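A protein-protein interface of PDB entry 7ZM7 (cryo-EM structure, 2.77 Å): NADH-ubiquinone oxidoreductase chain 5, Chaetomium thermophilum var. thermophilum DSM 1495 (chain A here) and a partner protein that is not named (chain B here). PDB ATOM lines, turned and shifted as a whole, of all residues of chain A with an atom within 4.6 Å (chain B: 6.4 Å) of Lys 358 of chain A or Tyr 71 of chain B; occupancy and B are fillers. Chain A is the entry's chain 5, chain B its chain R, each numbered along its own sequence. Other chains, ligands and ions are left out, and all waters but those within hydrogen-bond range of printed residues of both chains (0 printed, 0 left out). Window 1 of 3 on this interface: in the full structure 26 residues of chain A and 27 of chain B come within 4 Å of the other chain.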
ATOM      1  N   ASN A 353      30.861   7.760  22.565  1.00  0.00           N
ATOM      2  CA  ASN A 353      29.919   8.639  23.241  1.00  0.00           C
ATOM      3  C   ASN A 353      29.666   9.869  22.390  1.00  0.00           C
ATOM      4  O   ASN A 353      30.532  10.312  21.637  1.00  0.00           O
ATOM      5  CB  ASN A 353      30.453   9.069  24.605  1.00  0.00           C
ATOM      6  CG  ASN A 353      29.568  10.087  25.277  1.00  0.00           C
ATOM      7  OD1 ASN A 353      28.447   9.779  25.668  1.00  0.00           O
ATOM      8  ND2 ASN A 353      30.052  11.316  25.391  1.00  0.00           N
ATOM      9  N   ASP A 355      27.471  12.694  23.728  1.00  0.00           N
ATOM     10  CA  ASP A 355      26.819  13.735  24.502  1.00  0.00           C
ATOM     11  C   ASP A 355      27.785  14.856  24.848  1.00  0.00           C
ATOM     12  O   ASP A 355      28.930  14.614  25.229  1.00  0.00           O
ATOM     13  CB  ASP A 355      26.235  13.134  25.777  1.00  0.00           C
ATOM     14  CG  ASP A 355      25.119  13.944  26.335  1.00  0.00           C
ATOM     15  OD1 ASP A 355      25.365  15.087  26.747  1.00  0.00           O
ATOM     16  OD2 ASP A 355      23.985  13.442  26.363  1.00  0.00           O
ATOM     17  N   PHE A 356      27.356  16.104  24.731  1.00  0.00           N
ATOM     18  CA  PHE A 356      28.244  17.252  25.053  1.00  0.00           C
ATOM     19  C   PHE A 356      28.516  17.317  26.549  1.00  0.00           C
ATOM     20  O   PHE A 356      29.619  17.718  26.927  1.00  0.00           O
ATOM     21  CB  PHE A 356      27.547  18.585  24.786  1.00  0.00           C
ATOM     22  CG  PHE A 356      27.518  19.050  23.357  1.00  0.00           C
ATOM     23  CD1 PHE A 356      28.684  19.403  22.706  1.00  0.00           C
ATOM     24  CD2 PHE A 356      26.317  19.176  22.684  1.00  0.00           C
ATOM     25  CE1 PHE A 356      28.651  19.851  21.398  1.00  0.00           C
ATOM     26  CE2 PHE A 356      26.286  19.624  21.375  1.00  0.00           C
ATOM     27  CZ  PHE A 356      27.453  19.959  20.734  1.00  0.00           C
ATOM     28  N   ARG A 357      27.548  16.918  27.370  1.00  0.00           N
ATOM     29  CA  ARG A 357      27.666  17.069  28.842  1.00  0.00           C
ATOM     30  C   ARG A 357      28.848  16.269  29.373  1.00  0.00           C
ATOM     31  O   ARG A 357      29.383  16.672  30.409  1.00  0.00           O
ATOM     32  CB  ARG A 357      26.349  16.689  29.516  1.00  0.00           C
ATOM     33  CG  ARG A 357      25.225  17.676  29.248  1.00  0.00           C
ATOM     34  CD  ARG A 357      23.857  17.188  29.676  1.00  0.00           C
ATOM     35  NE  ARG A 357      23.325  16.209  28.743  1.00  0.00           N
ATOM     36  CZ  ARG A 357      22.085  15.741  28.781  1.00  0.00           C
ATOM     37  NH1 ARG A 357      21.244  16.172  29.705  1.00  0.00           N
ATOM     38  NH2 ARG A 357      21.685  14.855  27.888  1.00  0.00           N
ATOM     39  N   LYS A 358      29.184  15.151  28.736  1.00  0.00           N
ATOM     40  CA  LYS A 358      30.282  14.283  29.222  1.00  0.00           C
ATOM     41  C   LYS A 358      31.567  14.479  28.409  1.00  0.00           C
ATOM     42  O   LYS A 358      32.399  13.575  28.437  1.00  0.00           O
ATOM     43  CB  LYS A 358      29.798  12.835  29.333  1.00  0.00           C
ATOM     44  CG  LYS A 358      28.599  12.634  30.245  1.00  0.00           C
ATOM     45  CD  LYS A 358      28.858  13.029  31.682  1.00  0.00           C
ATOM     46  CE  LYS A 358      27.622  12.922  32.548  1.00  0.00           C
ATOM     47  NZ  LYS A 358      27.909  13.282  33.956  1.00  0.00           N
ATOM     48  N   PHE A 359      31.697  15.558  27.642  1.00  0.00           N
ATOM     49  CA  PHE A 359      32.983  15.857  26.951  1.00  0.00           C
ATOM     50  C   PHE A 359      33.544  17.151  27.529  1.00  0.00           C
ATOM     51  O   PHE A 359      32.733  18.069  27.788  1.00  0.00           O
ATOM     52  CB  PHE A 359      32.831  16.140  25.457  1.00  0.00           C
ATOM     53  CG  PHE A 359      32.425  14.986  24.578  1.00  0.00           C
ATOM     54  CD1 PHE A 359      33.012  13.742  24.723  1.00  0.00           C
ATOM     55  CD2 PHE A 359      31.487  15.164  23.575  1.00  0.00           C
ATOM     56  CE1 PHE A 359      32.642  12.691  23.900  1.00  0.00           C
ATOM     57  CE2 PHE A 359      31.118  14.112  22.756  1.00  0.00           C
ATOM     58  CZ  PHE A 359      31.699  12.879  22.918  1.00  0.00           C
ATOM     59  N   GLY A 360      34.855  17.204  27.754  1.00  0.00           N
ATOM     60  CA  GLY A 360      35.507  18.416  28.282  1.00  0.00           C
ATOM     61  C   GLY A 360      36.996  18.259  28.126  1.00  0.00           C
ATOM     62  O   GLY A 360      37.419  17.140  27.842  1.00  0.00           O
ATOM     63  N   ASN A 438      34.519  16.825  31.640  1.00  0.00           N
ATOM     64  CA  ASN A 438      33.175  16.473  32.168  1.00  0.00           C
ATOM     65  C   ASN A 438      32.961  14.956  32.139  1.00  0.00           C
ATOM     66  O   ASN A 438      32.132  14.476  32.927  1.00  0.00           O
ATOM     67  CB  ASN A 438      32.075  17.266  31.459  1.00  0.00           C
ATOM     68  CG  ASN A 438      31.768  18.585  32.133  1.00  0.00           C
ATOM     69  OD1 ASN A 438      32.306  18.887  33.196  1.00  0.00           O
ATOM     70  ND2 ASN A 438      30.897  19.375  31.527  1.00  0.00           N
ATOM     71  N   GLY A 439      33.686  14.230  31.300  1.00  0.00           N
ATOM     72  CA  GLY A 439      33.492  12.811  31.163  1.00  0.00           C
ATOM     73  C   GLY A 439      34.277  12.003  32.176  1.00  0.00           C
ATOM     74  O   GLY A 439      34.886  12.546  33.100  1.00  0.00           O
ATOM     75  N   TYR A 443      39.026   8.823  30.003  1.00  0.00           N
ATOM     76  CA  TYR A 443      39.206   9.643  28.810  1.00  0.00           C
ATOM     77  C   TYR A 443      40.497  10.433  28.868  1.00  0.00           C
ATOM     78  O   TYR A 443      41.010  10.855  27.828  1.00  0.00           O
ATOM     79  CB  TYR A 443      38.037  10.609  28.629  1.00  0.00           C
ATOM     80  CG  TYR A 443      36.759   9.964  28.177  1.00  0.00           C
ATOM     81  CD1 TYR A 443      36.768   8.761  27.500  1.00  0.00           C
ATOM     82  CD2 TYR A 443      35.542  10.567  28.425  1.00  0.00           C
ATOM     83  CE1 TYR A 443      35.595   8.171  27.090  1.00  0.00           C
ATOM     84  CE2 TYR A 443      34.366   9.989  28.020  1.00  0.00           C
ATOM     85  CZ  TYR A 443      34.395   8.792  27.353  1.00  0.00           C
ATOM     86  OH  TYR A 443      33.214   8.221  26.948  1.00  0.00           O
ATOM     87  N   LEU B  19      22.414  17.140  37.809  1.00  0.00           N
ATOM     88  CA  LEU B  19      23.601  17.037  36.925  1.00  0.00           C
ATOM     89  C   LEU B  19      23.182  17.393  35.510  1.00  0.00           C
ATOM     90  O   LEU B  19      23.985  17.964  34.777  1.00  0.00           O
ATOM     91  CB  LEU B  19      24.148  15.610  36.975  1.00  0.00           C
ATOM     92  CG  LEU B  19      25.579  15.429  36.474  1.00  0.00           C
ATOM     93  CD1 LEU B  19      26.445  16.619  36.846  1.00  0.00           C
ATOM     94  CD2 LEU B  19      26.178  14.143  37.016  1.00  0.00           C
ATOM     95  N   ASP B  20      21.990  16.967  35.119  1.00  0.00           N
ATOM     96  CA  ASP B  20      21.529  17.207  33.738  1.00  0.00           C
ATOM     97  C   ASP B  20      21.348  18.701  33.490  1.00  0.00           C
ATOM     98  O   ASP B  20      21.667  19.164  32.381  1.00  0.00           O
ATOM     99  CB  ASP B  20      20.279  16.387  33.454  1.00  0.00           C
ATOM    100  CG  ASP B  20      20.554  14.932  33.123  1.00  0.00           C
ATOM    101  OD1 ASP B  20      21.459  14.679  32.305  1.00  0.00           O
ATOM    102  OD2 ASP B  20      19.859  14.065  33.683  1.00  0.00           O
ATOM    103  N   ARG B  25      30.533  20.454  36.395  1.00  0.00           N
ATOM    104  CA  ARG B  25      30.505  19.514  37.510  1.00  0.00           C
ATOM    105  C   ARG B  25      30.766  20.202  38.840  1.00  0.00           C
ATOM    106  O   ARG B  25      30.182  19.822  39.859  1.00  0.00           O
ATOM    107  CB  ARG B  25      31.516  18.395  37.283  1.00  0.00           C
ATOM    108  CG  ARG B  25      30.995  17.279  36.408  1.00  0.00           C
ATOM    109  CD  ARG B  25      32.033  16.185  36.248  1.00  0.00           C
ATOM    110  NE  ARG B  25      32.230  15.411  37.474  1.00  0.00           N
ATOM    111  CZ  ARG B  25      31.303  14.656  38.058  1.00  0.00           C
ATOM    112  NH1 ARG B  25      30.090  14.541  37.533  1.00  0.00           N
ATOM    113  NH2 ARG B  25      31.597  13.999  39.169  1.00  0.00           N
ATOM    114  N   HIS B  67      14.260  16.858  33.081  1.00  0.00           N
ATOM    115  CA  HIS B  67      15.058  17.341  31.937  1.00  0.00           C
ATOM    116  C   HIS B  67      14.377  16.868  30.640  1.00  0.00           C
ATOM    117  O   HIS B  67      13.908  15.714  30.626  1.00  0.00           O
ATOM    118  CB  HIS B  67      16.492  16.846  32.104  1.00  0.00           C
ATOM    119  CG  HIS B  67      17.490  17.664  31.355  1.00  0.00           C
ATOM    120  ND1 HIS B  67      17.769  17.454  30.021  1.00  0.00           N
ATOM    121  CD2 HIS B  67      18.269  18.695  31.744  1.00  0.00           C
ATOM    122  CE1 HIS B  67      18.679  18.320  29.621  1.00  0.00           C
ATOM    123  NE2 HIS B  67      19.002  19.093  30.659  1.00  0.00           N
ATOM    124  N   ASP B  69      15.743  15.903  27.905  1.00  0.00           N
ATOM    125  CA  ASP B  69      16.524  14.737  27.506  1.00  0.00           C
ATOM    126  C   ASP B  69      17.587  14.419  28.550  1.00  0.00           C
ATOM    127  O   ASP B  69      18.692  14.982  28.524  1.00  0.00           O
ATOM    128  CB  ASP B  69      17.130  14.930  26.120  1.00  0.00           C
ATOM    129  CG  ASP B  69      17.907  16.223  25.993  1.00  0.00           C
ATOM    130  OD1 ASP B  69      17.872  17.037  26.938  1.00  0.00           O
ATOM    131  OD2 ASP B  69      18.549  16.423  24.940  1.00  0.00           O
ATOM    132  N   PRO B  70      17.271  13.543  29.551  1.00  0.00           N
ATOM    133  CA  PRO B  70      18.246  13.144  30.539  1.00  0.00           C
ATOM    134  C   PRO B  70      19.377  12.410  29.823  1.00  0.00           C
ATOM    135  O   PRO B  70      19.115  11.696  28.879  1.00  0.00           O
ATOM    136  CB  PRO B  70      17.526  12.120  31.404  1.00  0.00           C
ATOM    137  CG  PRO B  70      16.083  12.497  31.286  1.00  0.00           C
ATOM    138  CD  PRO B  70      15.974  12.878  29.830  1.00  0.00           C
ATOM    139  N   TYR B  71      20.602  12.600  30.297  1.00  0.00           N
ATOM    140  CA  TYR B  71      21.765  11.957  29.657  1.00  0.00           C
ATOM    141  C   TYR B  71      21.610  10.450  29.744  1.00  0.00           C
ATOM    142  O   TYR B  71      21.102   9.958  30.752  1.00  0.00           O
ATOM    143  CB  TYR B  71      23.049  12.387  30.375  1.00  0.00           C
ATOM    144  CG  TYR B  71      24.227  11.456  30.218  1.00  0.00           C
ATOM    145  CD1 TYR B  71      25.014  11.483  29.082  1.00  0.00           C
ATOM    146  CD2 TYR B  71      24.562  10.558  31.215  1.00  0.00           C
ATOM    147  CE1 TYR B  71      26.096  10.633  28.932  1.00  0.00           C
ATOM    148  CE2 TYR B  71      25.636   9.696  31.080  1.00  0.00           C
ATOM    149  CZ  TYR B  71      26.409   9.736  29.936  1.00  0.00           C
ATOM    150  OH  TYR B  71      27.474   8.895  29.801  1.00  0.00           O
ATOM    151  N   CYS B  72      22.039   9.749  28.700  1.00  0.00           N
ATOM    152  CA  CYS B  72      22.062   8.271  28.774  1.00  0.00           C
ATOM    153  C   CYS B  72      23.471   7.791  28.417  1.00  0.00           C
ATOM    154  O   CYS B  72      24.007   8.305  27.429  1.00  0.00           O
ATOM    155  CB  CYS B  72      21.035   7.621  27.859  1.00  0.00           C
ATOM    156  SG  CYS B  72      20.561   5.962  28.402  1.00  0.00           S
ATOM    157  N   PRO B  73      24.128   6.886  29.185  1.00  0.00           N
ATOM    158  CA  PRO B  73      25.395   6.322  28.750  1.00  0.00           C
ATOM    159  C   PRO B  73      25.226   5.661  27.398  1.00  0.00           C
ATOM    160  O   PRO B  73      24.180   5.054  27.127  1.00  0.00           O
ATOM    161  CB  PRO B  73      25.717   5.291  29.837  1.00  0.00           C
ATOM    162  CG  PRO B  73      24.901   5.683  30.991  1.00  0.00           C
ATOM    163  CD  PRO B  73      23.664   6.284  30.442  1.00  0.00           C
ATOM    164  N   PRO B  74      26.240   5.735  26.536  1.00  0.00           N
ATOM    165  CA  PRO B  74      26.047   5.359  25.131  1.00  0.00           C
ATOM    166  C   PRO B  74      25.641   3.926  24.926  1.00  0.00           C
ATOM    167  O   PRO B  74      25.126   3.582  23.859  1.00  0.00           O
ATOM    168  CB  PRO B  74      27.422   5.629  24.519  1.00  0.00           C
ATOM    169  CG  PRO B  74      28.047   6.578  25.419  1.00  0.00           C
ATOM    170  CD  PRO B  74      27.595   6.237  26.778  1.00  0.00           C
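Among the printed residues, merely in contact across the chains: Asn 353 of chain A with Pro 74 of chain B, Asp 355 of chain A with Tyr 71 of chain B, Arg 357 of chain A with His 67 of chain B, Arg 357 of chain A with Pro 70 of chain B, Lys 358 of chain A with Leu 19 of chain B, Lys 358 of chain A with Tyr 71 of chain B and Asn 438 of chain A with Arg 25 of chain B.
Of the 10 printed residues of chain B, 8 touch a printed residue of chain A. Hydrophobic or aromatic side chains of chain B that line the printed part of chain A: Leu 19, His 67, Tyr 71 and Pro 74. Among the printed residues, 10 pairs touch across the chains. Among the printed residues, Asp or Glu carboxylates within 4 Å of a Lys or Arg side-chain nitrogen of the other chain: Arg 357 of chain A with Asp 20 of chain B (3.0 Å).
The side-chain carboxylate (OD1) of Asp 355 of chain A is in salt-bridge range of the guanidinium group (NE) of Arg 357 of chain A, at 3.1 Å. The backbone carbonyl oxygen (O) of Lys 358 of chain A sits close to the backbone NH (N) of Gly 439 of chain A (3.2 Å). ND1 of His 67 of chain B lies within hydrogen-bond range of O of Asp 69 of chain B (3.0 Å). The side-chain carboxylate (OD1) of Asp 20 of chain B lies within hydrogen-bond range of the backbone NH (N) of Tyr 71 of chain B (3.0 Å). O of Arg 357 of chain A sits close to ND2 of Asn 438 of chain A. The backbone NH (N) of Asp 355 of chain A lies close to the side-chain amide nitrogen (ND2) of Asn 353 of chain A (3.4 Å).
Lys 358 of chain A touches two residues of chain B. Tyr 71 of chain B touches just these residues of chain A: Asp 355 (3.5 Å), Arg 357 (3.4 Å) and Lys 358 (3.5 Å). Printed residues of chain B within 4 Å of Asn 353 of chain A: Pro 74. Of the printed residues of chain A, His 67 of chain B touches Arg 357. The nearest residue of chain B that does not touch Lys 358 of chain A is Arg 25 of chain B (4.4 Å).
The backbone NH of Tyr 71 of chain B sits close to the guanidinium group of Arg 357 of chain A (3.5 Å). The guanidinium group (NH1) of Arg 357 of chain A lies within salt-bridge range of the side-chain carboxylate (OD1) of Asp 20 of chain B, 3.0 Å away. NH1 of Arg 357 of chain A is in hydrogen-bond range of O of Asp 69 of chain B (3.1 Å).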
